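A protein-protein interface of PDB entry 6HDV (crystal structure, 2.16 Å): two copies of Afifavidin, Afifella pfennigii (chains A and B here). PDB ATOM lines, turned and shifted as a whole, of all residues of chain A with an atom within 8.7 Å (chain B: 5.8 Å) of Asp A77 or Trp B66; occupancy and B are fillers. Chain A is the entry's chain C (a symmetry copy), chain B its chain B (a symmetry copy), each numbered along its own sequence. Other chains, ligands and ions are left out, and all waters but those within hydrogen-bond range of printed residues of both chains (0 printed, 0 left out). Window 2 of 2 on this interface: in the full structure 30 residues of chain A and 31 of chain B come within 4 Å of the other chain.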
ATOM      1  N   PHE A  44      21.438 -11.508 -15.710  1.00  0.00           N
ATOM      2  CA  PHE A  44      22.304 -10.885 -14.761  1.00  0.00           C
ATOM      3  C   PHE A  44      22.574  -9.467 -15.288  1.00  0.00           C
ATOM      4  O   PHE A  44      22.695  -9.267 -16.536  1.00  0.00           O
ATOM      5  CB  PHE A  44      23.586 -11.728 -14.546  1.00  0.00           C
ATOM      6  CG  PHE A  44      23.445 -12.950 -13.639  1.00  0.00           C
ATOM      7  CD1 PHE A  44      22.936 -14.166 -14.114  1.00  0.00           C
ATOM      8  CD2 PHE A  44      23.843 -12.913 -12.297  1.00  0.00           C
ATOM      9  CE1 PHE A  44      22.777 -15.272 -13.279  1.00  0.00           C
ATOM     10  CE2 PHE A  44      23.714 -14.026 -11.468  1.00  0.00           C
ATOM     11  CZ  PHE A  44      23.161 -15.195 -11.956  1.00  0.00           C
ATOM     12  N   PHE A  52      25.709   5.681  -8.703  1.00  0.00           N
ATOM     13  CA  PHE A  52      24.841   4.607  -8.208  1.00  0.00           C
ATOM     14  C   PHE A  52      25.721   3.730  -7.307  1.00  0.00           C
ATOM     15  O   PHE A  52      26.791   3.375  -7.733  1.00  0.00           O
ATOM     16  CB  PHE A  52      24.198   3.901  -9.410  1.00  0.00           C
ATOM     17  CG  PHE A  52      23.241   2.770  -9.101  1.00  0.00           C
ATOM     18  CD1 PHE A  52      23.716   1.471  -8.931  1.00  0.00           C
ATOM     19  CD2 PHE A  52      21.865   2.971  -9.049  1.00  0.00           C
ATOM     20  CE1 PHE A  52      22.857   0.426  -8.611  1.00  0.00           C
ATOM     21  CE2 PHE A  52      21.018   1.915  -8.752  1.00  0.00           C
ATOM     22  CZ  PHE A  52      21.512   0.655  -8.511  1.00  0.00           C
ATOM     23  N   CYS A  54      26.303  -0.033  -5.417  1.00  0.00           N
ATOM     24  CA  CYS A  54      26.028  -1.341  -6.070  1.00  0.00           C
ATOM     25  C   CYS A  54      26.501  -1.372  -7.535  1.00  0.00           C
ATOM     26  O   CYS A  54      25.890  -2.027  -8.360  1.00  0.00           O
ATOM     27  CB  CYS A  54      24.546  -1.724  -5.984  1.00  0.00           C
ATOM     28  SG  CYS A  54      24.020  -2.056  -4.285  1.00  0.00           S
ATOM     29  N   THR A  57      29.186  -5.230  -9.728  1.00  0.00           N
ATOM     30  CA  THR A  57      28.912  -6.694  -9.531  1.00  0.00           C
ATOM     31  C   THR A  57      27.575  -7.085 -10.143  1.00  0.00           C
ATOM     32  O   THR A  57      26.693  -6.259 -10.339  1.00  0.00           O
ATOM     33  CB  THR A  57      28.880  -7.153  -8.064  1.00  0.00           C
ATOM     34  OG1 THR A  57      27.890  -6.446  -7.317  1.00  0.00           O
ATOM     35  CG2 THR A  57      30.227  -7.000  -7.395  1.00  0.00           C
ATOM     36  N   PRO A  58      27.390  -8.365 -10.482  1.00  0.00           N
ATOM     37  CA  PRO A  58      26.141  -8.795 -11.081  1.00  0.00           C
ATOM     38  C   PRO A  58      25.050  -9.097 -10.041  1.00  0.00           C
ATOM     39  O   PRO A  58      25.303  -9.614  -8.918  1.00  0.00           O
ATOM     40  CB  PRO A  58      26.572 -10.017 -11.881  1.00  0.00           C
ATOM     41  CG  PRO A  58      27.712 -10.606 -11.065  1.00  0.00           C
ATOM     42  CD  PRO A  58      28.412  -9.422 -10.436  1.00  0.00           C
ATOM     43  N   TYR A  59      23.834  -8.678 -10.432  1.00  0.00           N
ATOM     44  CA  TYR A  59      22.607  -8.919  -9.737  1.00  0.00           C
ATOM     45  C   TYR A  59      21.661  -9.660 -10.677  1.00  0.00           C
ATOM     46  O   TYR A  59      21.639  -9.407 -11.881  1.00  0.00           O
ATOM     47  CB  TYR A  59      22.016  -7.575  -9.327  1.00  0.00           C
ATOM     48  CG  TYR A  59      22.806  -6.850  -8.283  1.00  0.00           C
ATOM     49  CD1 TYR A  59      23.907  -6.083  -8.620  1.00  0.00           C
ATOM     50  CD2 TYR A  59      22.465  -6.959  -6.952  1.00  0.00           C
ATOM     51  CE1 TYR A  59      24.649  -5.435  -7.646  1.00  0.00           C
ATOM     52  CE2 TYR A  59      23.216  -6.345  -5.960  1.00  0.00           C
ATOM     53  CZ  TYR A  59      24.311  -5.580  -6.313  1.00  0.00           C
ATOM     54  OH  TYR A  59      25.027  -4.958  -5.333  1.00  0.00           O
ATOM     55  N   PRO A  60      20.890 -10.650 -10.199  1.00  0.00           N
ATOM     56  CA  PRO A  60      19.984 -11.380 -11.086  1.00  0.00           C
ATOM     57  C   PRO A  60      18.837 -10.513 -11.623  1.00  0.00           C
ATOM     58  O   PRO A  60      18.396  -9.580 -10.935  1.00  0.00           O
ATOM     59  CB  PRO A  60      19.377 -12.492 -10.238  1.00  0.00           C
ATOM     60  CG  PRO A  60      20.146 -12.489  -8.920  1.00  0.00           C
ATOM     61  CD  PRO A  60      20.950 -11.201  -8.843  1.00  0.00           C
ATOM     62  N   LEU A  61      18.365 -10.843 -12.829  1.00  0.00           N
ATOM     63  CA  LEU A  61      17.217 -10.235 -13.348  1.00  0.00           C
ATOM     64  C   LEU A  61      16.237 -11.331 -13.772  1.00  0.00           C
ATOM     65  O   LEU A  61      16.659 -12.418 -14.142  1.00  0.00           O
ATOM     66  CB  LEU A  61      17.602  -9.295 -14.492  1.00  0.00           C
ATOM     67  CG  LEU A  61      18.040  -9.963 -15.789  1.00  0.00           C
ATOM     68  CD1 LEU A  61      16.871 -10.270 -16.708  1.00  0.00           C
ATOM     69  CD2 LEU A  61      19.028  -9.091 -16.525  1.00  0.00           C
ATOM     70  N   THR A  73      13.024  -6.985 -13.925  1.00  0.00           N
ATOM     71  CA  THR A  73      13.397  -6.278 -12.730  1.00  0.00           C
ATOM     72  C   THR A  73      14.672  -6.856 -12.103  1.00  0.00           C
ATOM     73  O   THR A  73      15.126  -7.992 -12.385  1.00  0.00           O
ATOM     74  CB  THR A  73      12.210  -6.103 -11.786  1.00  0.00           C
ATOM     75  OG1 THR A  73      12.524  -6.675 -10.531  1.00  0.00           O
ATOM     76  CG2 THR A  73      10.921  -6.627 -12.371  1.00  0.00           C
ATOM     77  N   VAL A  74      15.344  -5.969 -11.363  1.00  0.00           N
ATOM     78  CA  VAL A  74      16.546  -6.279 -10.651  1.00  0.00           C
ATOM     79  C   VAL A  74      16.337  -5.804  -9.215  1.00  0.00           C
ATOM     80  O   VAL A  74      15.972  -4.662  -9.020  1.00  0.00           O
ATOM     81  CB  VAL A  74      17.785  -5.598 -11.275  1.00  0.00           C
ATOM     82  CG1 VAL A  74      18.986  -5.630 -10.334  1.00  0.00           C
ATOM     83  CG2 VAL A  74      18.179  -6.189 -12.628  1.00  0.00           C
ATOM     84  N   ALA A  75      16.564  -6.682  -8.226  1.00  0.00           N
ATOM     85  CA  ALA A  75      16.685  -6.231  -6.841  1.00  0.00           C
ATOM     86  C   ALA A  75      18.161  -6.046  -6.515  1.00  0.00           C
ATOM     87  O   ALA A  75      18.980  -6.920  -6.743  1.00  0.00           O
ATOM     88  CB  ALA A  75      16.040  -7.184  -5.890  1.00  0.00           C
ATOM     89  N   TRP A  76      18.478  -4.897  -5.940  1.00  0.00           N
ATOM     90  CA  TRP A  76      19.836  -4.556  -5.647  1.00  0.00           C
ATOM     91  C   TRP A  76      20.229  -5.267  -4.366  1.00  0.00           C
ATOM     92  O   TRP A  76      20.454  -4.635  -3.329  1.00  0.00           O
ATOM     93  CB  TRP A  76      19.999  -3.040  -5.597  1.00  0.00           C
ATOM     94  CG  TRP A  76      19.578  -2.475  -6.911  1.00  0.00           C
ATOM     95  CD1 TRP A  76      18.442  -1.765  -7.189  1.00  0.00           C
ATOM     96  CD2 TRP A  76      20.225  -2.725  -8.168  1.00  0.00           C
ATOM     97  NE1 TRP A  76      18.377  -1.524  -8.533  1.00  0.00           N
ATOM     98  CE2 TRP A  76      19.447  -2.102  -9.157  1.00  0.00           C
ATOM     99  CE3 TRP A  76      21.364  -3.434  -8.544  1.00  0.00           C
ATOM    100  CZ2 TRP A  76      19.773  -2.146 -10.507  1.00  0.00           C
ATOM    101  CZ3 TRP A  76      21.695  -3.467  -9.877  1.00  0.00           C
ATOM    102  CH2 TRP A  76      20.915  -2.820 -10.841  1.00  0.00           C
ATOM    103  N   ASP A  77      20.311  -6.594  -4.501  1.00  0.00           N
ATOM    104  CA  ASP A  77      20.768  -7.472  -3.442  1.00  0.00           C
ATOM    105  C   ASP A  77      21.571  -8.638  -4.023  1.00  0.00           C
ATOM    106  O   ASP A  77      21.077  -9.373  -4.887  1.00  0.00           O
ATOM    107  CB  ASP A  77      19.598  -8.025  -2.647  1.00  0.00           C
ATOM    108  CG  ASP A  77      20.056  -8.980  -1.577  1.00  0.00           C
ATOM    109  OD1 ASP A  77      20.843  -8.526  -0.727  1.00  0.00           O
ATOM    110  OD2 ASP A  77      19.600 -10.148  -1.587  1.00  0.00           O
ATOM    111  N   ASN A  78      22.801  -8.787  -3.521  1.00  0.00           N
ATOM    112  CA  ASN A  78      23.690  -9.943  -3.776  1.00  0.00           C
ATOM    113  C   ASN A  78      24.714 -10.034  -2.629  1.00  0.00           C
ATOM    114  O   ASN A  78      24.650  -9.285  -1.645  1.00  0.00           O
ATOM    115  CB  ASN A  78      24.317  -9.889  -5.176  1.00  0.00           C
ATOM    116  CG  ASN A  78      25.406  -8.855  -5.344  1.00  0.00           C
ATOM    117  OD1 ASN A  78      25.836  -8.236  -4.362  1.00  0.00           O
ATOM    118  ND2 ASN A  78      25.846  -8.663  -6.594  1.00  0.00           N
ATOM    119  N   ALA A  79      25.654 -10.976  -2.751  1.00  0.00           N
ATOM    120  CA  ALA A  79      26.631 -11.269  -1.695  1.00  0.00           C
ATOM    121  C   ALA A  79      27.597 -10.100  -1.484  1.00  0.00           C
ATOM    122  O   ALA A  79      28.096  -9.912  -0.370  1.00  0.00           O
ATOM    123  CB  ALA A  79      27.384 -12.527  -2.030  1.00  0.00           C
ATOM    124  N   THR A  80      27.843  -9.308  -2.528  1.00  0.00           N
ATOM    125  CA  THR A  80      28.780  -8.158  -2.416  1.00  0.00           C
ATOM    126  C   THR A  80      28.159  -6.905  -1.754  1.00  0.00           C
ATOM    127  O   THR A  80      28.761  -6.294  -0.818  1.00  0.00           O
ATOM    128  CB  THR A  80      29.319  -7.749  -3.783  1.00  0.00           C
ATOM    129  OG1 THR A  80      29.743  -8.939  -4.463  1.00  0.00           O
ATOM    130  CG2 THR A  80      30.412  -6.717  -3.634  1.00  0.00           C
ATOM    131  N   ALA A  81      26.984  -6.479  -2.235  1.00  0.00           N
ATOM    132  CA  ALA A  81      26.382  -5.237  -1.730  1.00  0.00           C
ATOM    133  C   ALA A  81      24.875  -5.222  -1.963  1.00  0.00           C
ATOM    134  O   ALA A  81      24.390  -5.699  -3.007  1.00  0.00           O
ATOM    135  CB  ALA A  81      27.037  -4.032  -2.360  1.00  0.00           C
ATOM    136  N   ASN A  82      24.176  -4.695  -0.948  1.00  0.00           N
ATOM    137  CA  ASN A  82      22.720  -4.416  -0.954  1.00  0.00           C
ATOM    138  C   ASN A  82      22.445  -2.889  -0.929  1.00  0.00           C
ATOM    139  O   ASN A  82      22.944  -2.193  -0.068  1.00  0.00           O
ATOM    140  CB  ASN A  82      22.050  -5.094   0.246  1.00  0.00           C
ATOM    141  CG  ASN A  82      20.570  -4.798   0.339  1.00  0.00           C
ATOM    142  OD1 ASN A  82      19.752  -5.695   0.073  1.00  0.00           O
ATOM    143  ND2 ASN A  82      20.231  -3.548   0.680  1.00  0.00           N
ATOM    144  N   CYS A  83      21.590  -2.383  -1.826  1.00  0.00           N
ATOM    145  CA  CYS A  83      21.238  -0.938  -1.872  1.00  0.00           C
ATOM    146  C   CYS A  83      19.734  -0.697  -1.600  1.00  0.00           C
ATOM    147  O   CYS A  83      19.173   0.428  -1.859  1.00  0.00           O
ATOM    148  CB  CYS A  83      21.633  -0.353  -3.229  1.00  0.00           C
ATOM    149  SG  CYS A  83      23.425  -0.191  -3.465  1.00  0.00           S
ATOM    150  N   ASN A  84      19.037  -1.744  -1.135  1.00  0.00           N
ATOM    151  CA  ASN A  84      17.696  -1.615  -0.532  1.00  0.00           C
ATOM    152  C   ASN A  84      16.754  -0.888  -1.505  1.00  0.00           C
ATOM    153  O   ASN A  84      16.152   0.130  -1.176  1.00  0.00           O
ATOM    154  CB  ASN A  84      17.777  -0.920   0.830  1.00  0.00           C
ATOM    155  CG  ASN A  84      16.446  -0.818   1.532  1.00  0.00           C
ATOM    156  OD1 ASN A  84      15.627  -1.704   1.393  1.00  0.00           O
ATOM    157  ND2 ASN A  84      16.216   0.276   2.237  1.00  0.00           N
ATOM    158  N   SER A  85      16.618  -1.470  -2.700  1.00  0.00           N
ATOM    159  CA  SER A  85      15.924  -0.840  -3.794  1.00  0.00           C
ATOM    160  C   SER A  85      15.752  -1.855  -4.920  1.00  0.00           C
ATOM    161  O   SER A  85      16.455  -2.848  -4.978  1.00  0.00           O
ATOM    162  CB  SER A  85      16.704   0.357  -4.290  1.00  0.00           C
ATOM    163  OG  SER A  85      17.992  -0.049  -4.749  1.00  0.00           O
ATOM    164  N   VAL A  86      14.789  -1.613  -5.798  1.00  0.00           N
ATOM    165  CA  VAL A  86      14.667  -2.459  -6.948  1.00  0.00           C
ATOM    166  C   VAL A  86      14.300  -1.578  -8.136  1.00  0.00           C
ATOM    167  O   VAL A  86      13.667  -0.543  -7.945  1.00  0.00           O
ATOM    168  CB  VAL A  86      13.688  -3.645  -6.758  1.00  0.00           C
ATOM    169  CG1 VAL A  86      13.112  -3.755  -5.370  1.00  0.00           C
ATOM    170  CG2 VAL A  86      12.614  -3.695  -7.816  1.00  0.00           C
ATOM    171  N   THR A  87      14.702  -2.019  -9.331  1.00  0.00           N
ATOM    172  CA  THR A  87      14.489  -1.320 -10.558  1.00  0.00           C
ATOM    173  C   THR A  87      13.766  -2.237 -11.526  1.00  0.00           C
ATOM    174  O   THR A  87      14.122  -3.373 -11.596  1.00  0.00           O
ATOM    175  CB  THR A  87      15.824  -0.907 -11.190  1.00  0.00           C
ATOM    176  OG1 THR A  87      16.394   0.074 -10.343  1.00  0.00           O
ATOM    177  CG2 THR A  87      15.707  -0.358 -12.596  1.00  0.00           C
ATOM    178  N   ALA A 109      12.686   2.142  -7.313  1.00  0.00           N
ATOM    179  CA  ALA A 109      12.019   2.352  -6.051  1.00  0.00           C
ATOM    180  C   ALA A 109      13.038   2.149  -4.926  1.00  0.00           C
ATOM    181  O   ALA A 109      13.787   1.157  -4.957  1.00  0.00           O
ATOM    182  CB  ALA A 109      10.833   1.428  -5.922  1.00  0.00           C
ATOM    183  N   TYR A 110      13.065   3.090  -3.968  1.00  0.00           N
ATOM    184  CA  TYR A 110      14.143   3.166  -2.996  1.00  0.00           C
ATOM    185  C   TYR A 110      13.607   3.984  -1.836  1.00  0.00           C
ATOM    186  O   TYR A 110      12.514   4.479  -1.959  1.00  0.00           O
ATOM    187  CB  TYR A 110      15.430   3.745  -3.605  1.00  0.00           C
ATOM    188  CG  TYR A 110      15.406   5.234  -3.873  1.00  0.00           C
ATOM    189  CD1 TYR A 110      15.738   6.159  -2.898  1.00  0.00           C
ATOM    190  CD2 TYR A 110      14.993   5.734  -5.094  1.00  0.00           C
ATOM    191  CE1 TYR A 110      15.673   7.530  -3.141  1.00  0.00           C
ATOM    192  CE2 TYR A 110      14.921   7.098  -5.353  1.00  0.00           C
ATOM    193  CZ  TYR A 110      15.277   8.012  -4.378  1.00  0.00           C
ATOM    194  OH  TYR A 110      15.192   9.368  -4.626  1.00  0.00           O
ATOM    195  N   GLN B   3      21.318 -14.460   6.638  1.00  0.00           N
ATOM    196  CA  GLN B   3      21.778 -14.988   5.291  1.00  0.00           C
ATOM    197  C   GLN B   3      20.814 -14.438   4.207  1.00  0.00           C
ATOM    198  O   GLN B   3      20.967 -13.303   3.752  1.00  0.00           O
ATOM    199  CB  GLN B   3      21.982 -16.522   5.401  1.00  0.00           C
ATOM    200  CG  GLN B   3      22.306 -17.305   4.111  1.00  0.00           C
ATOM    201  CD  GLN B   3      23.295 -16.679   3.141  1.00  0.00           C
ATOM    202  OE1 GLN B   3      24.103 -15.828   3.503  1.00  0.00           O
ATOM    203  NE2 GLN B   3      23.240 -17.083   1.873  1.00  0.00           N
ATOM    204  N   MET B   5      16.587 -14.679   2.270  1.00  0.00           N
ATOM    205  CA  MET B   5      15.201 -14.581   2.748  1.00  0.00           C
ATOM    206  C   MET B   5      14.388 -15.806   2.307  1.00  0.00           C
ATOM    207  O   MET B   5      14.354 -16.155   1.123  1.00  0.00           O
ATOM    208  CB  MET B   5      14.505 -13.307   2.245  1.00  0.00           C
ATOM    209  CG  MET B   5      15.207 -12.000   2.658  1.00  0.00           C
ATOM    210  SD  MET B   5      15.455 -11.719   4.471  1.00  0.00           S
ATOM    211  CE  MET B   5      13.888 -11.012   4.967  1.00  0.00           C
ATOM    212  N   PHE B  14       8.172  -7.259   3.388  1.00  0.00           N
ATOM    213  CA  PHE B  14       7.474  -6.446   2.470  1.00  0.00           C
ATOM    214  C   PHE B  14       6.314  -5.791   3.192  1.00  0.00           C
ATOM    215  O   PHE B  14       5.937  -4.715   2.821  1.00  0.00           O
ATOM    216  CB  PHE B  14       6.948  -7.246   1.289  1.00  0.00           C
ATOM    217  CG  PHE B  14       6.260  -6.400   0.253  1.00  0.00           C
ATOM    218  CD1 PHE B  14       6.997  -5.552  -0.558  1.00  0.00           C
ATOM    219  CD2 PHE B  14       4.889  -6.468   0.071  1.00  0.00           C
ATOM    220  CE1 PHE B  14       6.376  -4.794  -1.535  1.00  0.00           C
ATOM    221  CE2 PHE B  14       4.270  -5.705  -0.906  1.00  0.00           C
ATOM    222  CZ  PHE B  14       5.007  -4.872  -1.711  1.00  0.00           C
ATOM    223  N   ASN B  39      14.444 -13.970  -3.410  1.00  0.00           N
ATOM    224  CA  ASN B  39      13.826 -12.658  -3.664  1.00  0.00           C
ATOM    225  C   ASN B  39      12.782 -12.726  -4.789  1.00  0.00           C
ATOM    226  O   ASN B  39      12.367 -11.694  -5.292  1.00  0.00           O
ATOM    227  CB  ASN B  39      14.889 -11.596  -3.968  1.00  0.00           C
ATOM    228  CG  ASN B  39      15.851 -11.440  -2.817  1.00  0.00           C
ATOM    229  OD1 ASN B  39      17.041 -11.256  -3.039  1.00  0.00           O
ATOM    230  ND2 ASN B  39      15.335 -11.521  -1.599  1.00  0.00           N
ATOM    231  N   LEU B  64      10.851  -9.377  -8.512  1.00  0.00           N
ATOM    232  CA  LEU B  64      11.700  -9.539  -7.388  1.00  0.00           C
ATOM    233  C   LEU B  64      11.337  -8.506  -6.333  1.00  0.00           C
ATOM    234  O   LEU B  64      10.767  -7.490  -6.651  1.00  0.00           O
ATOM    235  CB  LEU B  64      13.165  -9.362  -7.809  1.00  0.00           C
ATOM    236  CG  LEU B  64      13.680 -10.368  -8.836  1.00  0.00           C
ATOM    237  CD1 LEU B  64      15.075  -9.984  -9.306  1.00  0.00           C
ATOM    238  CD2 LEU B  64      13.681 -11.779  -8.250  1.00  0.00           C
ATOM    239  N   THR B  65      11.768  -8.776  -5.103  1.00  0.00           N
ATOM    240  CA  THR B  65      11.600  -7.893  -3.975  1.00  0.00           C
ATOM    241  C   THR B  65      12.875  -7.838  -3.160  1.00  0.00           C
ATOM    242  O   THR B  65      13.639  -8.788  -3.150  1.00  0.00           O
ATOM    243  CB  THR B  65      10.585  -8.398  -2.955  1.00  0.00           C
ATOM    244  OG1 THR B  65      10.692  -9.822  -2.771  1.00  0.00           O
ATOM    245  CG2 THR B  65       9.207  -8.048  -3.419  1.00  0.00           C
ATOM    246  N   TRP B  66      12.990  -6.739  -2.422  1.00  0.00           N
ATOM    247  CA  TRP B  66      13.780  -6.673  -1.245  1.00  0.00           C
ATOM    248  C   TRP B  66      13.090  -5.704  -0.290  1.00  0.00           C
ATOM    249  O   TRP B  66      12.603  -4.641  -0.710  1.00  0.00           O
ATOM    250  CB  TRP B  66      15.207  -6.209  -1.569  1.00  0.00           C
ATOM    251  CG  TRP B  66      16.010  -6.093  -0.316  1.00  0.00           C
ATOM    252  CD1 TRP B  66      16.147  -5.022   0.518  1.00  0.00           C
ATOM    253  CD2 TRP B  66      16.633  -7.189   0.353  1.00  0.00           C
ATOM    254  NE1 TRP B  66      16.863  -5.358   1.639  1.00  0.00           N
ATOM    255  CE2 TRP B  66      17.189  -6.683   1.552  1.00  0.00           C
ATOM    256  CE3 TRP B  66      16.766  -8.545   0.033  1.00  0.00           C
ATOM    257  CZ2 TRP B  66      17.883  -7.499   2.435  1.00  0.00           C
ATOM    258  CZ3 TRP B  66      17.456  -9.346   0.906  1.00  0.00           C
ATOM    259  CH2 TRP B  66      18.008  -8.826   2.085  1.00  0.00           C
ATOM    260  N   GLY B  67      13.094  -6.030   0.993  1.00  0.00           N
ATOM    261  CA  GLY B  67      12.491  -5.157   1.973  1.00  0.00           C
ATOM    262  C   GLY B  67      11.100  -4.744   1.527  1.00  0.00           C
ATOM    263  O   GLY B  67      10.379  -5.597   1.049  1.00  0.00           O
ATOM    264  N   ASN B  68      10.787  -3.440   1.623  1.00  0.00           N
ATOM    265  CA  ASN B  68       9.513  -2.857   1.218  1.00  0.00           C
ATOM    266  C   ASN B  68       9.376  -2.720  -0.310  1.00  0.00           C
ATOM    267  O   ASN B  68       8.331  -2.302  -0.779  1.00  0.00           O
ATOM    268  CB  ASN B  68       9.347  -1.413   1.685  1.00  0.00           C
ATOM    269  CG  ASN B  68       9.556  -1.230   3.162  1.00  0.00           C
ATOM    270  OD1 ASN B  68       8.971  -1.932   3.977  1.00  0.00           O
ATOM    271  ND2 ASN B  68      10.377  -0.263   3.499  1.00  0.00           N
ATOM    272  N   PHE B  69      10.429  -3.015  -1.074  1.00  0.00           N
ATOM    273  CA  PHE B  69      10.523  -2.667  -2.480  1.00  0.00           C
ATOM    274  C   PHE B  69      10.228  -3.879  -3.362  1.00  0.00           C
ATOM    275  O   PHE B  69      10.595  -5.057  -3.050  1.00  0.00           O
ATOM    276  CB  PHE B  69      11.892  -2.024  -2.765  1.00  0.00           C
ATOM    277  CG  PHE B  69      12.103  -0.795  -1.916  1.00  0.00           C
ATOM    278  CD1 PHE B  69      11.319   0.332  -2.119  1.00  0.00           C
ATOM    279  CD2 PHE B  69      12.992  -0.810  -0.846  1.00  0.00           C
ATOM    280  CE1 PHE B  69      11.436   1.428  -1.281  1.00  0.00           C
ATOM    281  CE2 PHE B  69      13.121   0.293  -0.018  1.00  0.00           C
ATOM    282  CZ  PHE B  69      12.340   1.407  -0.234  1.00  0.00           C
ATOM    283  N   ILE B  70       9.624  -3.574  -4.516  1.00  0.00           N
ATOM    284  CA  ILE B  70       9.149  -4.601  -5.413  1.00  0.00           C
ATOM    285  C   ILE B  70       9.174  -4.102  -6.853  1.00  0.00           C
ATOM    286  O   ILE B  70       8.884  -2.966  -7.138  1.00  0.00           O
ATOM    287  CB  ILE B  70       7.729  -5.058  -5.011  1.00  0.00           C
ATOM    288  CG1 ILE B  70       7.311  -6.332  -5.736  1.00  0.00           C
ATOM    289  CG2 ILE B  70       6.685  -3.982  -5.234  1.00  0.00           C
ATOM    290  CD1 ILE B  70       6.348  -7.179  -4.930  1.00  0.00           C
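ND2 of Asn A82 lies close to N of Asn A84 (2.8 Å). The backbone carbonyl oxygen of Asn B39 sits at hydrogen-bond distance from the backbone NH of Thr B65. SG of Cys A83 is disulfide-bonded to SG of Cys A54, at 2.1 Å. The side-chain carboxylate (OD1) of Asp A77 lies close to the side-chain amide oxygen (OD1) of Asn A82, at 3.1 Å. The backbone NH of Ala A109 sits at hydrogen-bond distance from the backbone carbonyl oxygen of Val A86.
Among the printed residues, pairs that only touch across the chains: Asn A84 with Phe B69 (3.2 Å), Tyr A110 with Phe B69 (3.3 Å), Val A86 with Phe B69 (3.4 Å), Asp A77 with Trp B66 (3.4 Å), Asn A84 with Trp B66 (3.5 Å), Val A86 with Ile B70 (3.6 Å), Thr A73 with Leu B64 (3.7 Å), Pro A60 with Leu B64 (3.7 Å), Ala A109 with Phe B69 (3.8 Å), Ala A75 with Leu B64 (3.8 Å) and Ala A75 with Thr B65 (3.98 Å).
No position is printed for both chains. Of the 13 pairs that touch across the chains among the printed residues, none has its exchanged pair printed and touching as well.
Of the 11 printed residues of chain B, 6 touch a printed residue of chain A. Hydrophobic or aromatic side chains of chain B that line the printed part of chain A: Leu B64, Trp B66 and Phe B69. Hydrophobic or aromatic side chains of chain A within 4 Å of the printed part of chain B: Ala A75, Val A86 and Ala A109. Among the printed residues, no Asp or Glu carboxylate lies within 4 Å of a Lys or Arg side-chain nitrogen of the other chain.
Of chain B, only Asn B39 and Trp B66 come within 4 Å of Asp A77. Trp B66 touches just these residues of chain A: Asp A77 (3.4 Å), Asn A82 (3.1 Å) and Asn A84 (3.5 Å). Printed residues of chain B within 4 Å of Ala A109: Phe B69 (3.8 Å). Of the printed residues of chain B, Asn A84 touches Trp B66 and Phe B69. Of the printed residues of chain B, Tyr A110 touches Phe B69. Phe B14 touches none of the printed residues of chain A. Val A74 touches none of the printed residues of chain B. The nearest residue of chain A that does not touch Trp B66 is Val A86 (4.2 Å). The nearest printed residue of chain B that does not touch Thr A73 is Ile B70 (5.6 Å).
NE1 of Trp B66 sits close to OD1 of Asn A82, at 3.3 Å. OD1 of Asn B39 sits close to OD2 of Asp A77 (3.1 Å).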
